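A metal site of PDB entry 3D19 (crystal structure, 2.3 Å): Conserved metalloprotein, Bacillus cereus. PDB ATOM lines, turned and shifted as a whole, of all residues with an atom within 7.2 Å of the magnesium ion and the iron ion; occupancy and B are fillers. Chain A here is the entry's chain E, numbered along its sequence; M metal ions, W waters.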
ATOM      1  N   TRP A  23      31.983  38.192   1.286  1.00  0.00           N
ATOM      2  CA  TRP A  23      31.343  38.112  -0.033  1.00  0.00           C
ATOM      3  C   TRP A  23      32.268  38.391  -1.239  1.00  0.00           C
ATOM      4  O   TRP A  23      32.098  37.795  -2.300  1.00  0.00           O
ATOM      5  CB  TRP A  23      30.080  38.953  -0.108  1.00  0.00           C
ATOM      6  CG  TRP A  23      28.969  38.391   0.758  1.00  0.00           C
ATOM      7  CD1 TRP A  23      28.474  38.928   1.905  1.00  0.00           C
ATOM      8  CD2 TRP A  23      28.232  37.181   0.536  1.00  0.00           C
ATOM      9  NE1 TRP A  23      27.477  38.151   2.417  1.00  0.00           N
ATOM     10  CE2 TRP A  23      27.308  37.063   1.598  1.00  0.00           C
ATOM     11  CE3 TRP A  23      28.261  36.182  -0.459  1.00  0.00           C
ATOM     12  CZ2 TRP A  23      26.414  35.970   1.699  1.00  0.00           C
ATOM     13  CZ3 TRP A  23      27.381  35.109  -0.352  1.00  0.00           C
ATOM     14  CH2 TRP A  23      26.482  35.017   0.716  1.00  0.00           C
ATOM     15  N   ILE A  26      33.620  35.175  -2.094  1.00  0.00           N
ATOM     16  CA  ILE A  26      32.544  34.412  -2.755  1.00  0.00           C
ATOM     17  C   ILE A  26      32.433  34.783  -4.248  1.00  0.00           C
ATOM     18  O   ILE A  26      32.381  33.915  -5.090  1.00  0.00           O
ATOM     19  CB  ILE A  26      31.178  34.595  -2.026  1.00  0.00           C
ATOM     20  CG1 ILE A  26      31.232  34.104  -0.545  1.00  0.00           C
ATOM     21  CG2 ILE A  26      30.089  33.878  -2.787  1.00  0.00           C
ATOM     22  CD1 ILE A  26      31.622  32.623  -0.346  1.00  0.00           C
ATOM     23  N   MET A  27      32.444  36.083  -4.567  1.00  0.00           N
ATOM     24  CA  MET A  27      32.374  36.568  -5.967  1.00  0.00           C
ATOM     25  C   MET A  27      33.630  36.233  -6.754  1.00  0.00           C
ATOM     26  O   MET A  27      33.571  35.781  -7.917  1.00  0.00           O
ATOM     27  CB  MET A  27      32.094  38.078  -6.042  1.00  0.00           C
ATOM     28  CG  MET A  27      30.797  38.526  -5.329  1.00  0.00           C
ATOM     29  SD  MET A  27      29.210  37.984  -6.054  1.00  0.00           S
ATOM     30  CE  MET A  27      28.423  37.333  -4.570  1.00  0.00           C
ATOM     31  N   GLU A  29      35.284  33.760  -6.256  1.00  0.00           N
ATOM     32  CA  GLU A  29      35.248  32.320  -6.445  1.00  0.00           C
ATOM     33  C   GLU A  29      34.252  31.902  -7.538  1.00  0.00           C
ATOM     34  O   GLU A  29      34.596  31.069  -8.372  1.00  0.00           O
ATOM     35  CB  GLU A  29      35.092  31.597  -5.092  1.00  0.00           C
ATOM     36  CG  GLU A  29      36.433  31.583  -4.308  1.00  0.00           C
ATOM     37  CD  GLU A  29      36.346  31.060  -2.877  1.00  0.00           C
ATOM     38  OE1 GLU A  29      37.424  30.734  -2.300  1.00  0.00           O
ATOM     39  OE2 GLU A  29      35.203  30.974  -2.323  1.00  0.00           O
ATOM     40  N   HIS A  30      33.067  32.512  -7.560  1.00  0.00           N
ATOM     41  CA  HIS A  30      32.123  32.273  -8.674  1.00  0.00           C
ATOM     42  C   HIS A  30      32.705  32.481 -10.031  1.00  0.00           C
ATOM     43  O   HIS A  30      32.514  31.655 -10.939  1.00  0.00           O
ATOM     44  CB  HIS A  30      30.900  33.148  -8.568  1.00  0.00           C
ATOM     45  CG  HIS A  30      30.077  32.857  -7.370  1.00  0.00           C
ATOM     46  ND1 HIS A  30      29.209  33.777  -6.826  1.00  0.00           N
ATOM     47  CD2 HIS A  30      29.975  31.754  -6.608  1.00  0.00           C
ATOM     48  CE1 HIS A  30      28.607  33.253  -5.776  1.00  0.00           C
ATOM     49  NE2 HIS A  30      29.059  32.022  -5.610  1.00  0.00           N
ATOM     50  N   PHE A  33      34.579  29.406 -10.777  1.00  0.00           N
ATOM     51  CA  PHE A  33      33.687  28.265 -10.989  1.00  0.00           C
ATOM     52  C   PHE A  33      32.982  28.375 -12.336  1.00  0.00           C
ATOM     53  O   PHE A  33      32.882  27.393 -13.050  1.00  0.00           O
ATOM     54  CB  PHE A  33      32.691  28.096  -9.840  1.00  0.00           C
ATOM     55  CG  PHE A  33      33.353  27.840  -8.499  1.00  0.00           C
ATOM     56  CD1 PHE A  33      34.465  26.998  -8.410  1.00  0.00           C
ATOM     57  CD2 PHE A  33      32.886  28.462  -7.342  1.00  0.00           C
ATOM     58  CE1 PHE A  33      35.092  26.784  -7.197  1.00  0.00           C
ATOM     59  CE2 PHE A  33      33.503  28.237  -6.138  1.00  0.00           C
ATOM     60  CZ  PHE A  33      34.601  27.409  -6.060  1.00  0.00           C
ATOM     61  N   LYS A  93      26.317  37.174 -14.754  1.00  0.00           N
ATOM     62  CA  LYS A  93      25.732  35.876 -14.447  1.00  0.00           C
ATOM     63  C   LYS A  93      24.350  35.794 -15.111  1.00  0.00           C
ATOM     64  O   LYS A  93      23.976  34.760 -15.610  1.00  0.00           O
ATOM     65  CB  LYS A  93      25.645  35.687 -12.937  1.00  0.00           C
ATOM     66  CG  LYS A  93      27.010  35.401 -12.281  1.00  0.00           C
ATOM     67  CD  LYS A  93      27.010  35.814 -10.798  1.00  0.00           C
ATOM     68  CE  LYS A  93      28.350  35.407 -10.097  1.00  0.00           C
ATOM     69  NZ  LYS A  93      28.379  35.778  -8.628  1.00  0.00           N
ATOM     70  N   LEU A 114      22.748  26.652 -10.825  1.00  0.00           N
ATOM     71  CA  LEU A 114      24.005  27.229 -10.349  1.00  0.00           C
ATOM     72  C   LEU A 114      24.044  28.724 -10.730  1.00  0.00           C
ATOM     73  O   LEU A 114      24.221  29.579  -9.877  1.00  0.00           O
ATOM     74  CB  LEU A 114      25.222  26.482 -10.938  1.00  0.00           C
ATOM     75  CG  LEU A 114      26.560  27.138 -10.527  1.00  0.00           C
ATOM     76  CD1 LEU A 114      26.929  26.751  -9.123  1.00  0.00           C
ATOM     77  CD2 LEU A 114      27.675  26.807 -11.476  1.00  0.00           C
ATOM     78  N   HIS A 117      21.699  30.888  -8.956  1.00  0.00           N
ATOM     79  CA  HIS A 117      22.119  30.847  -7.558  1.00  0.00           C
ATOM     80  C   HIS A 117      23.277  31.838  -7.218  1.00  0.00           C
ATOM     81  O   HIS A 117      23.215  32.580  -6.236  1.00  0.00           O
ATOM     82  CB  HIS A 117      22.537  29.414  -7.270  1.00  0.00           C
ATOM     83  CG  HIS A 117      23.049  29.168  -5.887  1.00  0.00           C
ATOM     84  ND1 HIS A 117      22.263  28.618  -4.891  1.00  0.00           N
ATOM     85  CD2 HIS A 117      24.287  29.334  -5.360  1.00  0.00           C
ATOM     86  CE1 HIS A 117      22.993  28.473  -3.800  1.00  0.00           C
ATOM     87  NE2 HIS A 117      24.218  28.920  -4.041  1.00  0.00           N
ATOM     88  N   THR A 118      24.358  31.823  -7.995  1.00  0.00           N
ATOM     89  CA  THR A 118      25.419  32.844  -7.877  1.00  0.00           C
ATOM     90  C   THR A 118      24.806  34.231  -8.024  1.00  0.00           C
ATOM     91  O   THR A 118      25.115  35.176  -7.272  1.00  0.00           O
ATOM     92  CB  THR A 118      26.475  32.649  -8.977  1.00  0.00           C
ATOM     93  OG1 THR A 118      25.894  32.841 -10.282  1.00  0.00           O
ATOM     94  CG2 THR A 118      27.103  31.269  -8.912  1.00  0.00           C
ATOM     95  N   GLU A 121      22.997  35.179  -4.808  1.00  0.00           N
ATOM     96  CA  GLU A 121      24.042  35.538  -3.809  1.00  0.00           C
ATOM     97  C   GLU A 121      24.624  36.919  -4.114  1.00  0.00           C
ATOM     98  O   GLU A 121      24.729  37.774  -3.224  1.00  0.00           O
ATOM     99  CB  GLU A 121      25.139  34.483  -3.775  1.00  0.00           C
ATOM    100  CG  GLU A 121      24.745  33.221  -3.016  1.00  0.00           C
ATOM    101  CD  GLU A 121      25.864  32.170  -2.978  1.00  0.00           C
ATOM    102  OE1 GLU A 121      26.948  32.416  -3.542  1.00  0.00           O
ATOM    103  OE2 GLU A 121      25.657  31.092  -2.344  1.00  0.00           O
ATOM    104  N   ALA A 122      24.990  37.124  -5.359  1.00  0.00           N
ATOM    105  CA  ALA A 122      25.476  38.410  -5.855  1.00  0.00           C
ATOM    106  C   ALA A 122      24.518  39.546  -5.549  1.00  0.00           C
ATOM    107  O   ALA A 122      24.945  40.620  -5.125  1.00  0.00           O
ATOM    108  CB  ALA A 122      25.731  38.321  -7.364  1.00  0.00           C
ATOM    109  N   ILE A 154      19.519  28.586  -0.493  1.00  0.00           N
ATOM    110  CA  ILE A 154      20.944  28.343  -0.772  1.00  0.00           C
ATOM    111  C   ILE A 154      21.456  27.006  -0.213  1.00  0.00           C
ATOM    112  O   ILE A 154      22.122  26.220  -0.891  1.00  0.00           O
ATOM    113  CB  ILE A 154      21.764  29.530  -0.241  1.00  0.00           C
ATOM    114  CG1 ILE A 154      21.730  30.647  -1.276  1.00  0.00           C
ATOM    115  CG2 ILE A 154      23.176  29.160   0.004  1.00  0.00           C
ATOM    116  CD1 ILE A 154      20.689  31.637  -0.988  1.00  0.00           C
ATOM    117  N   MET A 155      21.108  26.720   1.023  1.00  0.00           N
ATOM    118  CA  MET A 155      21.377  25.407   1.565  1.00  0.00           C
ATOM    119  C   MET A 155      20.726  24.314   0.670  1.00  0.00           C
ATOM    120  O   MET A 155      21.377  23.342   0.287  1.00  0.00           O
ATOM    121  CB  MET A 155      20.858  25.331   2.999  1.00  0.00           C
ATOM    122  CG  MET A 155      21.551  26.306   4.016  1.00  0.00           C
ATOM    123  SD  MET A 155      23.303  25.962   4.187  1.00  0.00           S
ATOM    124  CE  MET A 155      23.976  27.452   3.474  1.00  0.00           C
ATOM    125  N   ASP A 157      19.883  24.343  -2.534  1.00  0.00           N
ATOM    126  CA  ASP A 157      20.551  24.201  -3.841  1.00  0.00           C
ATOM    127  C   ASP A 157      21.873  23.459  -3.693  1.00  0.00           C
ATOM    128  O   ASP A 157      22.232  22.613  -4.516  1.00  0.00           O
ATOM    129  CB  ASP A 157      20.833  25.549  -4.502  1.00  0.00           C
ATOM    130  CG  ASP A 157      19.542  26.407  -4.761  1.00  0.00           C
ATOM    131  OD1 ASP A 157      18.402  25.886  -4.784  1.00  0.00           O
ATOM    132  OD2 ASP A 157      19.697  27.639  -4.988  1.00  0.00           O
ATOM    133  N   HIS A 158      22.631  23.802  -2.657  1.00  0.00           N
ATOM    134  CA  HIS A 158      23.979  23.205  -2.439  1.00  0.00           C
ATOM    135  C   HIS A 158      23.947  21.679  -2.322  1.00  0.00           C
ATOM    136  O   HIS A 158      24.793  20.972  -2.881  1.00  0.00           O
ATOM    137  CB  HIS A 158      24.564  23.727  -1.140  1.00  0.00           C
ATOM    138  CG  HIS A 158      25.101  25.122  -1.232  1.00  0.00           C
ATOM    139  ND1 HIS A 158      25.364  25.892  -0.107  1.00  0.00           N
ATOM    140  CD2 HIS A 158      25.382  25.897  -2.303  1.00  0.00           C
ATOM    141  CE1 HIS A 158      25.792  27.082  -0.497  1.00  0.00           C
ATOM    142  NE2 HIS A 158      25.836  27.099  -1.822  1.00  0.00           N
ATOM    143  N   PHE A 161      23.643  20.501  -5.781  1.00  0.00           N
ATOM    144  CA  PHE A 161      24.932  20.591  -6.516  1.00  0.00           C
ATOM    145  C   PHE A 161      25.878  19.512  -6.045  1.00  0.00           C
ATOM    146  O   PHE A 161      26.585  18.883  -6.807  1.00  0.00           O
ATOM    147  CB  PHE A 161      25.606  21.952  -6.300  1.00  0.00           C
ATOM    148  CG  PHE A 161      24.742  23.112  -6.660  1.00  0.00           C
ATOM    149  CD1 PHE A 161      23.845  23.024  -7.724  1.00  0.00           C
ATOM    150  CD2 PHE A 161      24.861  24.319  -5.967  1.00  0.00           C
ATOM    151  CE1 PHE A 161      23.030  24.090  -8.066  1.00  0.00           C
ATOM    152  CE2 PHE A 161      24.059  25.404  -6.280  1.00  0.00           C
ATOM    153  CZ  PHE A 161      23.128  25.303  -7.324  1.00  0.00           C
ATOM    154  N   LYS A 225      29.555  18.982   4.641  1.00  0.00           N
ATOM    155  CA  LYS A 225      30.332  19.747   3.680  1.00  0.00           C
ATOM    156  C   LYS A 225      31.816  19.771   4.052  1.00  0.00           C
ATOM    157  O   LYS A 225      32.698  19.591   3.208  1.00  0.00           O
ATOM    158  CB  LYS A 225      29.799  21.174   3.654  1.00  0.00           C
ATOM    159  CG  LYS A 225      28.627  21.330   2.739  1.00  0.00           C
ATOM    160  CD  LYS A 225      28.076  22.736   2.872  1.00  0.00           C
ATOM    161  CE  LYS A 225      26.899  22.904   1.950  1.00  0.00           C
ATOM    162  NZ  LYS A 225      26.066  24.042   2.328  1.00  0.00           N
ATOM    163  N   LEU A 245      35.265  24.454  -4.548  1.00  0.00           N
ATOM    164  CA  LEU A 245      33.812  24.578  -4.474  1.00  0.00           C
ATOM    165  C   LEU A 245      33.288  24.012  -3.165  1.00  0.00           C
ATOM    166  O   LEU A 245      32.458  24.624  -2.514  1.00  0.00           O
ATOM    167  CB  LEU A 245      33.136  23.824  -5.640  1.00  0.00           C
ATOM    168  CG  LEU A 245      31.596  23.907  -5.723  1.00  0.00           C
ATOM    169  CD1 LEU A 245      31.071  25.340  -5.584  1.00  0.00           C
ATOM    170  CD2 LEU A 245      31.083  23.291  -7.008  1.00  0.00           C
ATOM    171  N   HIS A 248      33.934  26.343  -0.586  1.00  0.00           N
ATOM    172  CA  HIS A 248      33.019  27.475  -0.841  1.00  0.00           C
ATOM    173  C   HIS A 248      31.646  27.291  -0.223  1.00  0.00           C
ATOM    174  O   HIS A 248      31.175  28.176   0.497  1.00  0.00           O
ATOM    175  CB  HIS A 248      32.917  27.737  -2.366  1.00  0.00           C
ATOM    176  CG  HIS A 248      32.008  28.863  -2.769  1.00  0.00           C
ATOM    177  ND1 HIS A 248      32.467  29.994  -3.413  1.00  0.00           N
ATOM    178  CD2 HIS A 248      30.666  29.016  -2.652  1.00  0.00           C
ATOM    179  CE1 HIS A 248      31.441  30.801  -3.669  1.00  0.00           C
ATOM    180  NE2 HIS A 248      30.345  30.232  -3.228  1.00  0.00           N
ATOM    181  N   VAL A 249      31.006  26.159  -0.469  1.00  0.00           N
ATOM    182  CA  VAL A 249      29.706  25.879   0.188  1.00  0.00           C
ATOM    183  C   VAL A 249      29.849  25.694   1.685  1.00  0.00           C
ATOM    184  O   VAL A 249      28.986  26.118   2.438  1.00  0.00           O
ATOM    185  CB  VAL A 249      28.892  24.751  -0.478  1.00  0.00           C
ATOM    186  CG1 VAL A 249      28.700  25.048  -1.980  1.00  0.00           C
ATOM    187  CG2 VAL A 249      29.552  23.425  -0.304  1.00  0.00           C
ATOM    188  N   GLU A 252      29.769  29.141   3.205  1.00  0.00           N
ATOM    189  CA  GLU A 252      28.406  29.679   3.167  1.00  0.00           C
ATOM    190  C   GLU A 252      27.507  29.006   4.229  1.00  0.00           C
ATOM    191  O   GLU A 252      26.682  29.653   4.887  1.00  0.00           O
ATOM    192  CB  GLU A 252      27.841  29.585   1.773  1.00  0.00           C
ATOM    193  CG  GLU A 252      28.527  30.541   0.764  1.00  0.00           C
ATOM    194  CD  GLU A 252      28.092  30.336  -0.683  1.00  0.00           C
ATOM    195  OE1 GLU A 252      27.112  29.582  -0.943  1.00  0.00           O
ATOM    196  OE2 GLU A 252      28.691  30.966  -1.590  1.00  0.00           O
HETATM  197 MG    MG M   1      26.286  29.296  -2.560  1.00  0.00          MG
HETATM  198 FE    FE M   2      28.329  31.007  -3.688  1.00  0.00          FE
HETATM  199  O   HOH W   1      27.473  28.607  -4.307  1.00  0.00           O
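The magnesium ion is bound by OE1 of Glu 252 (1.8 Å), OE2 of Glu 121 (1.9 Å), water W1 (2.2 Å), NE2 of His 158 (2.4 Å) and NE2 of His 117 (2.6 Å). The magnesium ion has five donor atoms within binding distance.
The iron ion is bound by OE1 of Glu 121 (2.0 Å). The side-chain carboxylate (OE2) of Glu 252 binds the iron ion, at 2.1 Å. NE2 of His 248 binds the iron ion, at 2.2 Å. A ring nitrogen (NE2) of His 30 binds the iron ion. The iron ion has four donor atoms within binding distance. Slightly farther from the iron ion lies water W1 (2.6 Å).
Along chain A the residues within 4 Å of the magnesium ion span positions 117 to 252. The nearest printed residue that does not touch the magnesium ion is Ile 154 (4.03 Å).
The side-chain carboxylate of Glu 29 is in hydrogen-bond range of a ring nitrogen (ND1) of His 248 (3.1 Å). ND1 of His 158 lies within hydrogen-bond range of NZ of Lys 225, at 3.1 Å. The side-chain amino group of Lys 93 lies within hydrogen-bond range of a ring nitrogen (ND1) of His 30, 2.8 Å away. ND1 of His 158 lies close to O of Ile 154, at 3.4 Å. A ring nitrogen (ND1) of His 117 is in hydrogen-bond range of the side-chain carboxylate (OD2) of Asp 157 (2.7 Å).
Residues that only touch the iron ion: Ile 26 (3.5 Å). Of the 22 residues printed, 5 come within 4 Å of the iron ion.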
